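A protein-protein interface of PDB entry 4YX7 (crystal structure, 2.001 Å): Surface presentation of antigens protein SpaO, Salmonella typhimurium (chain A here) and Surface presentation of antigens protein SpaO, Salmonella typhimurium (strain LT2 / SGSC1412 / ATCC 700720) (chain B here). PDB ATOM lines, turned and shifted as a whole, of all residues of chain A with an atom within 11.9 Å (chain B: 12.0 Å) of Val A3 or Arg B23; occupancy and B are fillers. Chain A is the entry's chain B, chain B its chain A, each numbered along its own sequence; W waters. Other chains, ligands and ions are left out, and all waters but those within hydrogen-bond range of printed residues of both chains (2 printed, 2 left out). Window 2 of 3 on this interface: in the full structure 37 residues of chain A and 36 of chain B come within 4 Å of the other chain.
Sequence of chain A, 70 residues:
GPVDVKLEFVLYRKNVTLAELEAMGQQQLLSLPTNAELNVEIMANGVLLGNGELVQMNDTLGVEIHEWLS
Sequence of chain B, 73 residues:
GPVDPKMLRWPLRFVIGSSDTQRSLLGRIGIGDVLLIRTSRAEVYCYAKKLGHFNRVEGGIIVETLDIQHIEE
Val A3 touches Thr B21 (O to O, 3.9 Å). Gln B22 touches Val A3 (CA to O, 3.4 Å). CA of Asp A4 touches O of Thr B21, at 3.3 Å. O of Ser B19 touches O of Val A5 (3.8 Å). CG of Arg B23 touches CB of Val A5 (3.9 Å). C of Lys A6 touches O of Ser B19, 3.8 Å away. CA of Lys A6 touches OD1 of Asp B20 (3.4 Å). Thr B21 touches Leu A7 (OG1 to CD1, 3.2 Å). Leu B35 touches Leu A7 (CD1 to CD1, 3.9 Å). Trp A68 touches Ile B29.
Of chain A, only Val A3 (2.8 Å), Asp A4 (3.1 Å) and Val A5 (3.9 Å) come within 4 Å of Arg B23. Asp A4 touches two residues of chain B. Val A5 touches four residues of chain B. Thr B21 touches just these residues of chain A: Val A3 (3.9 Å), Asp A4 (3.3 Å), Val A5 (2.5 Å) and Leu A7 (3.2 Å). No residue of chain A comes within 4 Å of Ser B24. No residue of chain A comes within 4 Å of Leu B25. Leu B26 touches one residue of chain A. Of the printed residues of chain B, Trp A68 touches Leu B26 and Ile B29. Printed residues of chain A within 4 Å of Ile B29: Trp A68. Of the printed residues of chain A, Ser B19 touches Val A5, Lys A6 and Leu A7. Asn A45 touches none of the printed residues of chain B. The nearest residue of chain A that does not touch Arg B23 is Asn A45 (4.6 Å).
The backbone carbonyl oxygen (O) of Ser B19 is in hydrogen-bond range of the side-chain hydroxyl (OG1) of Thr B21. The side-chain hydroxyl (OG) of Ser B24 is in hydrogen-bond range of the side-chain amide nitrogen (NE2) of Gln B22 (3.1 Å).
The backbone NH of Leu A7 lies within hydrogen-bond range of the backbone carbonyl oxygen of Ser B19 (2.8 Å). N of Thr B21 is in hydrogen-bond range of O of Val A5, 2.5 Å away. The backbone NH (N) of Arg B23 is in hydrogen-bond range of the backbone carbonyl oxygen (O) of Val A3. The backbone carbonyl oxygen of Asp A4 is in hydrogen-bond range of the guanidinium group of Arg B23 (3.1 Å). The backbone carbonyl oxygen of Val A5 lies close to the side-chain carboxylate of Asp B20 (3.4 Å).
Of the 13 printed residues of chain B, 8 touch a printed residue of chain A. Along chain B the printed residues that touch a printed residue of chain A span positions 19 to 35. Of the 13 printed residues of chain A, 6 touch a printed residue of chain B. Hydrophobic or aromatic side chains of chain A that line the printed part of chain B: Val A3, Val A5, Leu A7 and Trp A68.
Water W2 bridges OD1 of Asp B20 (2.6 Å) and OD2 of Asp A4 (3.4 Å). Water W1 lies within hydrogen-bond range of N of Val A3 (2.7 Å) and OG of Ser B24 (2.9 Å).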
ATOM      1  N   VAL A   3     -33.707  12.284 -22.632  1.00  0.00           N
ATOM      2  CA  VAL A   3     -32.661  11.290 -22.424  1.00  0.00           C
ATOM      3  C   VAL A   3     -31.331  11.974 -22.080  1.00  0.00           C
ATOM      4  O   VAL A   3     -31.233  13.206 -22.091  1.00  0.00           O
ATOM      5  CB  VAL A   3     -32.510  10.382 -23.655  1.00  0.00           C
ATOM      6  CG1 VAL A   3     -33.866   9.962 -24.136  1.00  0.00           C
ATOM      7  CG2 VAL A   3     -31.777  11.082 -24.760  1.00  0.00           C
ATOM      8  N   ASP A   4     -30.308  11.173 -21.784  1.00  0.00           N
ATOM      9  CA  ASP A   4     -29.107  11.686 -21.115  1.00  0.00           C
ATOM     10  C   ASP A   4     -27.848  11.805 -21.974  1.00  0.00           C
ATOM     11  O   ASP A   4     -27.554  10.952 -22.806  1.00  0.00           O
ATOM     12  CB  ASP A   4     -28.781  10.817 -19.887  1.00  0.00           C
ATOM     13  CG  ASP A   4     -28.472   9.352 -20.240  1.00  0.00           C
ATOM     14  OD1 ASP A   4     -28.615   8.939 -21.416  1.00  0.00           O
ATOM     15  OD2 ASP A   4     -28.088   8.603 -19.315  1.00  0.00           O
ATOM     16  N   VAL A   5     -27.105  12.882 -21.739  1.00  0.00           N
ATOM     17  CA  VAL A   5     -25.778  13.070 -22.311  1.00  0.00           C
ATOM     18  C   VAL A   5     -24.800  13.221 -21.155  1.00  0.00           C
ATOM     19  O   VAL A   5     -25.148  13.767 -20.108  1.00  0.00           O
ATOM     20  CB  VAL A   5     -25.700  14.313 -23.260  1.00  0.00           C
ATOM     21  CG1 VAL A   5     -25.987  15.599 -22.521  1.00  0.00           C
ATOM     22  CG2 VAL A   5     -24.340  14.410 -23.936  1.00  0.00           C
ATOM     23  N   LYS A   6     -23.584  12.717 -21.326  1.00  0.00           N
ATOM     24  CA  LYS A   6     -22.575  12.830 -20.285  1.00  0.00           C
ATOM     25  C   LYS A   6     -21.655  14.031 -20.527  1.00  0.00           C
ATOM     26  O   LYS A   6     -20.884  14.039 -21.482  1.00  0.00           O
ATOM     27  CB  LYS A   6     -21.767  11.540 -20.203  1.00  0.00           C
ATOM     28  CG  LYS A   6     -20.649  11.600 -19.213  1.00  0.00           C
ATOM     29  CD  LYS A   6     -20.260  10.218 -18.799  1.00  0.00           C
ATOM     30  CE  LYS A   6     -18.887  10.235 -18.212  1.00  0.00           C
ATOM     31  NZ  LYS A   6     -17.902  10.397 -19.302  1.00  0.00           N
ATOM     32  N   LEU A   7     -21.758  15.048 -19.671  1.00  0.00           N
ATOM     33  CA  LEU A   7     -20.875  16.210 -19.747  1.00  0.00           C
ATOM     34  C   LEU A   7     -19.567  15.961 -19.007  1.00  0.00           C
ATOM     35  O   LEU A   7     -19.565  15.561 -17.852  1.00  0.00           O
ATOM     36  CB  LEU A   7     -21.548  17.461 -19.174  1.00  0.00           C
ATOM     37  CG  LEU A   7     -22.688  18.122 -19.953  1.00  0.00           C
ATOM     38  CD1 LEU A   7     -23.102  19.418 -19.278  1.00  0.00           C
ATOM     39  CD2 LEU A   7     -22.306  18.381 -21.389  1.00  0.00           C
ATOM     40  N   MET A  43     -17.186  19.440 -22.077  1.00  0.00           N
ATOM     41  CA  MET A  43     -17.246  18.645 -23.291  1.00  0.00           C
ATOM     42  C   MET A  43     -18.296  17.563 -23.165  1.00  0.00           C
ATOM     43  O   MET A  43     -18.570  17.086 -22.069  1.00  0.00           O
ATOM     44  CB  MET A  43     -15.876  18.047 -23.589  1.00  0.00           C
ATOM     45  CG  MET A  43     -14.787  19.095 -23.648  1.00  0.00           C
ATOM     46  SD  MET A  43     -13.265  18.376 -24.212  1.00  0.00           S
ATOM     47  CE  MET A  43     -13.534  18.261 -25.971  1.00  0.00           C
ATOM     48  N   ALA A  44     -18.895  17.179 -24.284  1.00  0.00           N
ATOM     49  CA  ALA A  44     -19.973  16.195 -24.229  1.00  0.00           C
ATOM     50  C   ALA A  44     -19.563  14.869 -24.841  1.00  0.00           C
ATOM     51  O   ALA A  44     -19.303  13.890 -24.125  1.00  0.00           O
ATOM     52  CB  ALA A  44     -21.207  16.728 -24.914  1.00  0.00           C
ATOM     53  N   ASN A  45     -19.507  14.835 -26.165  1.00  0.00           N
ATOM     54  CA  ASN A  45     -19.207  13.592 -26.872  1.00  0.00           C
ATOM     55  C   ASN A  45     -17.948  13.751 -27.701  1.00  0.00           C
ATOM     56  O   ASN A  45     -17.940  13.432 -28.891  1.00  0.00           O
ATOM     57  CB  ASN A  45     -20.372  13.170 -27.777  1.00  0.00           C
ATOM     58  CG  ASN A  45     -21.578  12.662 -26.998  1.00  0.00           C
ATOM     59  OD1 ASN A  45     -21.454  11.840 -26.090  1.00  0.00           O
ATOM     60  ND2 ASN A  45     -22.755  13.140 -27.368  1.00  0.00           N
ATOM     61  N   GLY A  46     -16.891  14.252 -27.067  1.00  0.00           N
ATOM     62  CA  GLY A  46     -15.669  14.571 -27.772  1.00  0.00           C
ATOM     63  C   GLY A  46     -15.733  15.973 -28.340  1.00  0.00           C
ATOM     64  O   GLY A  46     -14.771  16.465 -28.917  1.00  0.00           O
ATOM     65  N   VAL A  47     -16.870  16.629 -28.181  1.00  0.00           N
ATOM     66  CA  VAL A  47     -17.020  17.980 -28.696  1.00  0.00           C
ATOM     67  C   VAL A  47     -17.020  18.973 -27.543  1.00  0.00           C
ATOM     68  O   VAL A  47     -17.693  18.774 -26.530  1.00  0.00           O
ATOM     69  CB  VAL A  47     -18.319  18.157 -29.533  1.00  0.00           C
ATOM     70  CG1 VAL A  47     -18.203  19.379 -30.448  1.00  0.00           C
ATOM     71  CG2 VAL A  47     -18.583  16.935 -30.366  1.00  0.00           C
ATOM     72  N   LEU A  49     -18.108  22.180 -25.715  1.00  0.00           N
ATOM     73  CA  LEU A  49     -19.390  22.891 -25.673  1.00  0.00           C
ATOM     74  C   LEU A  49     -19.247  24.296 -25.095  1.00  0.00           C
ATOM     75  O   LEU A  49     -19.981  25.209 -25.462  1.00  0.00           O
ATOM     76  CB  LEU A  49     -20.421  22.111 -24.850  1.00  0.00           C
ATOM     77  CG  LEU A  49     -20.815  20.701 -25.305  1.00  0.00           C
ATOM     78  CD1 LEU A  49     -21.994  20.208 -24.494  1.00  0.00           C
ATOM     79  CD2 LEU A  49     -21.136  20.649 -26.782  1.00  0.00           C
ATOM     80  N   TRP A  68     -20.453  29.569 -23.884  1.00  0.00           N
ATOM     81  CA  TRP A  68     -21.258  28.413 -24.208  1.00  0.00           C
ATOM     82  C   TRP A  68     -21.664  28.452 -25.683  1.00  0.00           C
ATOM     83  O   TRP A  68     -22.409  29.344 -26.096  1.00  0.00           O
ATOM     84  CB  TRP A  68     -22.485  28.363 -23.308  1.00  0.00           C
ATOM     85  CG  TRP A  68     -23.183  27.023 -23.315  1.00  0.00           C
ATOM     86  CD1 TRP A  68     -24.392  26.725 -23.866  1.00  0.00           C
ATOM     87  CD2 TRP A  68     -22.692  25.808 -22.744  1.00  0.00           C
ATOM     88  NE1 TRP A  68     -24.686  25.392 -23.673  1.00  0.00           N
ATOM     89  CE2 TRP A  68     -23.656  24.809 -22.985  1.00  0.00           C
ATOM     90  CE3 TRP A  68     -21.526  25.467 -22.056  1.00  0.00           C
ATOM     91  CZ2 TRP A  68     -23.493  23.495 -22.554  1.00  0.00           C
ATOM     92  CZ3 TRP A  68     -21.367  24.157 -21.631  1.00  0.00           C
ATOM     93  CH2 TRP A  68     -22.342  23.193 -21.876  1.00  0.00           C
ATOM     94  N   LEU A  69     -21.145  27.500 -26.468  1.00  0.00           N
ATOM     95  CA  LEU A  69     -21.503  27.320 -27.885  1.00  0.00           C
ATOM     96  C   LEU A  69     -21.309  28.576 -28.738  1.00  0.00           C
ATOM     97  O   LEU A  69     -20.184  29.033 -28.946  1.00  0.00           O
ATOM     98  CB  LEU A  69     -22.952  26.849 -28.009  1.00  0.00           C
ATOM     99  CG  LEU A  69     -23.348  25.639 -27.165  1.00  0.00           C
ATOM    100  CD1 LEU A  69     -24.808  25.311 -27.376  1.00  0.00           C
ATOM    101  CD2 LEU A  69     -22.486  24.442 -27.504  1.00  0.00           C
ATOM    102  N   SER B  19     -20.876  15.031 -15.353  1.00  0.00           N
ATOM    103  CA  SER B  19     -22.264  15.152 -14.953  1.00  0.00           C
ATOM    104  C   SER B  19     -23.145  14.636 -16.071  1.00  0.00           C
ATOM    105  O   SER B  19     -23.076  15.133 -17.187  1.00  0.00           O
ATOM    106  CB  SER B  19     -22.615  16.603 -14.640  1.00  0.00           C
ATOM    107  OG  SER B  19     -22.151  16.985 -13.362  1.00  0.00           O
ATOM    108  N   ASP B  20     -23.974  13.638 -15.789  1.00  0.00           N
ATOM    109  CA  ASP B  20     -24.959  13.216 -16.774  1.00  0.00           C
ATOM    110  C   ASP B  20     -26.085  14.245 -16.885  1.00  0.00           C
ATOM    111  O   ASP B  20     -26.801  14.523 -15.916  1.00  0.00           O
ATOM    112  CB  ASP B  20     -25.519  11.842 -16.429  1.00  0.00           C
ATOM    113  CG  ASP B  20     -24.849  10.727 -17.209  1.00  0.00           C
ATOM    114  OD1 ASP B  20     -24.647  10.901 -18.433  1.00  0.00           O
ATOM    115  OD2 ASP B  20     -24.538   9.672 -16.609  1.00  0.00           O
ATOM    116  N   THR B  21     -26.226  14.804 -18.083  1.00  0.00           N
ATOM    117  CA  THR B  21     -27.146  15.912 -18.354  1.00  0.00           C
ATOM    118  C   THR B  21     -28.310  15.468 -19.240  1.00  0.00           C
ATOM    119  O   THR B  21     -28.137  14.721 -20.204  1.00  0.00           O
ATOM    120  CB  THR B  21     -26.446  17.072 -19.043  1.00  0.00           C
ATOM    121  OG1 THR B  21     -25.389  17.515 -18.200  1.00  0.00           O
ATOM    122  CG2 THR B  21     -27.424  18.242 -19.303  1.00  0.00           C
ATOM    123  N   GLN B  22     -29.498  15.955 -18.935  1.00  0.00           N
ATOM    124  CA  GLN B  22     -30.642  15.480 -19.637  1.00  0.00           C
ATOM    125  C   GLN B  22     -30.460  16.416 -20.852  1.00  0.00           C
ATOM    126  O   GLN B  22     -30.192  17.615 -20.664  1.00  0.00           O
ATOM    127  CB  GLN B  22     -31.901  15.644 -18.760  1.00  0.00           C
ATOM    128  CG  GLN B  22     -33.287  15.218 -19.263  1.00  0.00           C
ATOM    129  CD  GLN B  22     -34.313  16.214 -18.713  1.00  0.00           C
ATOM    130  OE1 GLN B  22     -33.990  17.006 -17.809  1.00  0.00           O
ATOM    131  NE2 GLN B  22     -35.569  16.102 -19.158  1.00  0.00           N
ATOM    132  N   ARG B  23     -30.556  15.894 -22.080  1.00  0.00           N
ATOM    133  CA  ARG B  23     -30.245  16.723 -23.243  1.00  0.00           C
ATOM    134  C   ARG B  23     -31.192  17.919 -23.327  1.00  0.00           C
ATOM    135  O   ARG B  23     -30.922  18.895 -24.023  1.00  0.00           O
ATOM    136  CB  ARG B  23     -30.293  15.906 -24.526  1.00  0.00           C
ATOM    137  CG  ARG B  23     -29.351  14.726 -24.538  1.00  0.00           C
ATOM    138  CD  ARG B  23     -29.626  13.830 -25.711  1.00  0.00           C
ATOM    139  NE  ARG B  23     -29.030  12.513 -25.532  1.00  0.00           N
ATOM    140  CZ  ARG B  23     -27.952  12.072 -26.171  1.00  0.00           C
ATOM    141  NH1 ARG B  23     -27.327  12.837 -27.052  1.00  0.00           N
ATOM    142  NH2 ARG B  23     -27.502  10.850 -25.931  1.00  0.00           N
ATOM    143  N   SER B  24     -32.276  17.861 -22.563  1.00  0.00           N
ATOM    144  CA  SER B  24     -33.248  18.944 -22.523  1.00  0.00           C
ATOM    145  C   SER B  24     -32.704  20.218 -21.877  1.00  0.00           C
ATOM    146  O   SER B  24     -33.336  21.274 -21.959  1.00  0.00           O
ATOM    147  CB  SER B  24     -34.494  18.490 -21.771  1.00  0.00           C
ATOM    148  OG  SER B  24     -34.739  17.110 -21.990  1.00  0.00           O
ATOM    149  N   LEU B  25     -31.547  20.116 -21.224  1.00  0.00           N
ATOM    150  CA  LEU B  25     -30.946  21.268 -20.554  1.00  0.00           C
ATOM    151  C   LEU B  25     -30.292  22.198 -21.553  1.00  0.00           C
ATOM    152  O   LEU B  25     -30.441  23.408 -21.462  1.00  0.00           O
ATOM    153  CB  LEU B  25     -29.927  20.831 -19.506  1.00  0.00           C
ATOM    154  CG  LEU B  25     -30.539  20.580 -18.126  1.00  0.00           C
ATOM    155  CD1 LEU B  25     -31.457  19.357 -18.135  1.00  0.00           C
ATOM    156  CD2 LEU B  25     -29.476  20.463 -17.062  1.00  0.00           C
ATOM    157  N   LEU B  26     -29.561  21.629 -22.502  1.00  0.00           N
ATOM    158  CA  LEU B  26     -29.096  22.385 -23.655  1.00  0.00           C
ATOM    159  C   LEU B  26     -30.261  22.536 -24.634  1.00  0.00           C
ATOM    160  O   LEU B  26     -30.824  21.536 -25.090  1.00  0.00           O
ATOM    161  CB  LEU B  26     -27.929  21.675 -24.329  1.00  0.00           C
ATOM    162  CG  LEU B  26     -27.114  20.821 -23.365  1.00  0.00           C
ATOM    163  CD1 LEU B  26     -26.140  19.917 -24.077  1.00  0.00           C
ATOM    164  CD2 LEU B  26     -26.384  21.742 -22.465  1.00  0.00           C
ATOM    165  N   GLY B  27     -30.626  23.768 -24.975  1.00  0.00           N
ATOM    166  CA  GLY B  27     -29.924  24.942 -24.521  1.00  0.00           C
ATOM    167  C   GLY B  27     -30.757  25.834 -23.622  1.00  0.00           C
ATOM    168  O   GLY B  27     -31.348  26.817 -24.065  1.00  0.00           O
ATOM    169  N   ARG B  28     -30.810  25.480 -22.346  1.00  0.00           N
ATOM    170  CA  ARG B  28     -31.222  26.430 -21.330  1.00  0.00           C
ATOM    171  C   ARG B  28     -29.972  27.002 -20.659  1.00  0.00           C
ATOM    172  O   ARG B  28     -29.988  28.133 -20.157  1.00  0.00           O
ATOM    173  CB  ARG B  28     -32.158  25.779 -20.310  1.00  0.00           C
ATOM    174  CG  ARG B  28     -33.519  25.388 -20.889  1.00  0.00           C
ATOM    175  CD  ARG B  28     -34.401  24.617 -19.886  1.00  0.00           C
ATOM    176  NE  ARG B  28     -34.527  25.277 -18.581  1.00  0.00           N
ATOM    177  CZ  ARG B  28     -34.915  26.538 -18.390  1.00  0.00           C
ATOM    178  NH1 ARG B  28     -35.256  27.313 -19.416  1.00  0.00           N
ATOM    179  NH2 ARG B  28     -34.984  27.030 -17.161  1.00  0.00           N
ATOM    180  N   ILE B  29     -28.894  26.218 -20.682  1.00  0.00           N
ATOM    181  CA  ILE B  29     -27.602  26.636 -20.157  1.00  0.00           C
ATOM    182  C   ILE B  29     -27.088  27.867 -20.885  1.00  0.00           C
ATOM    183  O   ILE B  29     -27.047  27.899 -22.111  1.00  0.00           O
ATOM    184  CB  ILE B  29     -26.557  25.515 -20.275  1.00  0.00           C
ATOM    185  CG1 ILE B  29     -27.056  24.250 -19.591  1.00  0.00           C
ATOM    186  CG2 ILE B  29     -25.238  25.947 -19.677  1.00  0.00           C
ATOM    187  CD1 ILE B  29     -26.048  23.174 -19.499  1.00  0.00           C
ATOM    188  N   GLY B  30     -26.704  28.882 -20.121  1.00  0.00           N
ATOM    189  CA  GLY B  30     -26.146  30.095 -20.685  1.00  0.00           C
ATOM    190  C   GLY B  30     -25.018  30.657 -19.841  1.00  0.00           C
ATOM    191  O   GLY B  30     -24.645  30.087 -18.822  1.00  0.00           O
ATOM    192  N   LEU B  35     -22.846  24.948 -13.559  1.00  0.00           N
ATOM    193  CA  LEU B  35     -23.066  23.524 -13.747  1.00  0.00           C
ATOM    194  C   LEU B  35     -22.404  22.762 -12.623  1.00  0.00           C
ATOM    195  O   LEU B  35     -21.196  22.827 -12.474  1.00  0.00           O
ATOM    196  CB  LEU B  35     -22.495  23.046 -15.080  1.00  0.00           C
ATOM    197  CG  LEU B  35     -23.034  23.661 -16.363  1.00  0.00           C
ATOM    198  CD1 LEU B  35     -22.483  22.891 -17.569  1.00  0.00           C
ATOM    199  CD2 LEU B  35     -24.545  23.663 -16.354  1.00  0.00           C
HETATM  200  O   HOH W   1     -33.898  14.806 -23.502  1.00  0.00           O
HETATM  201  O   HOH W   2     -24.668   8.640 -19.747  1.00  0.00           O
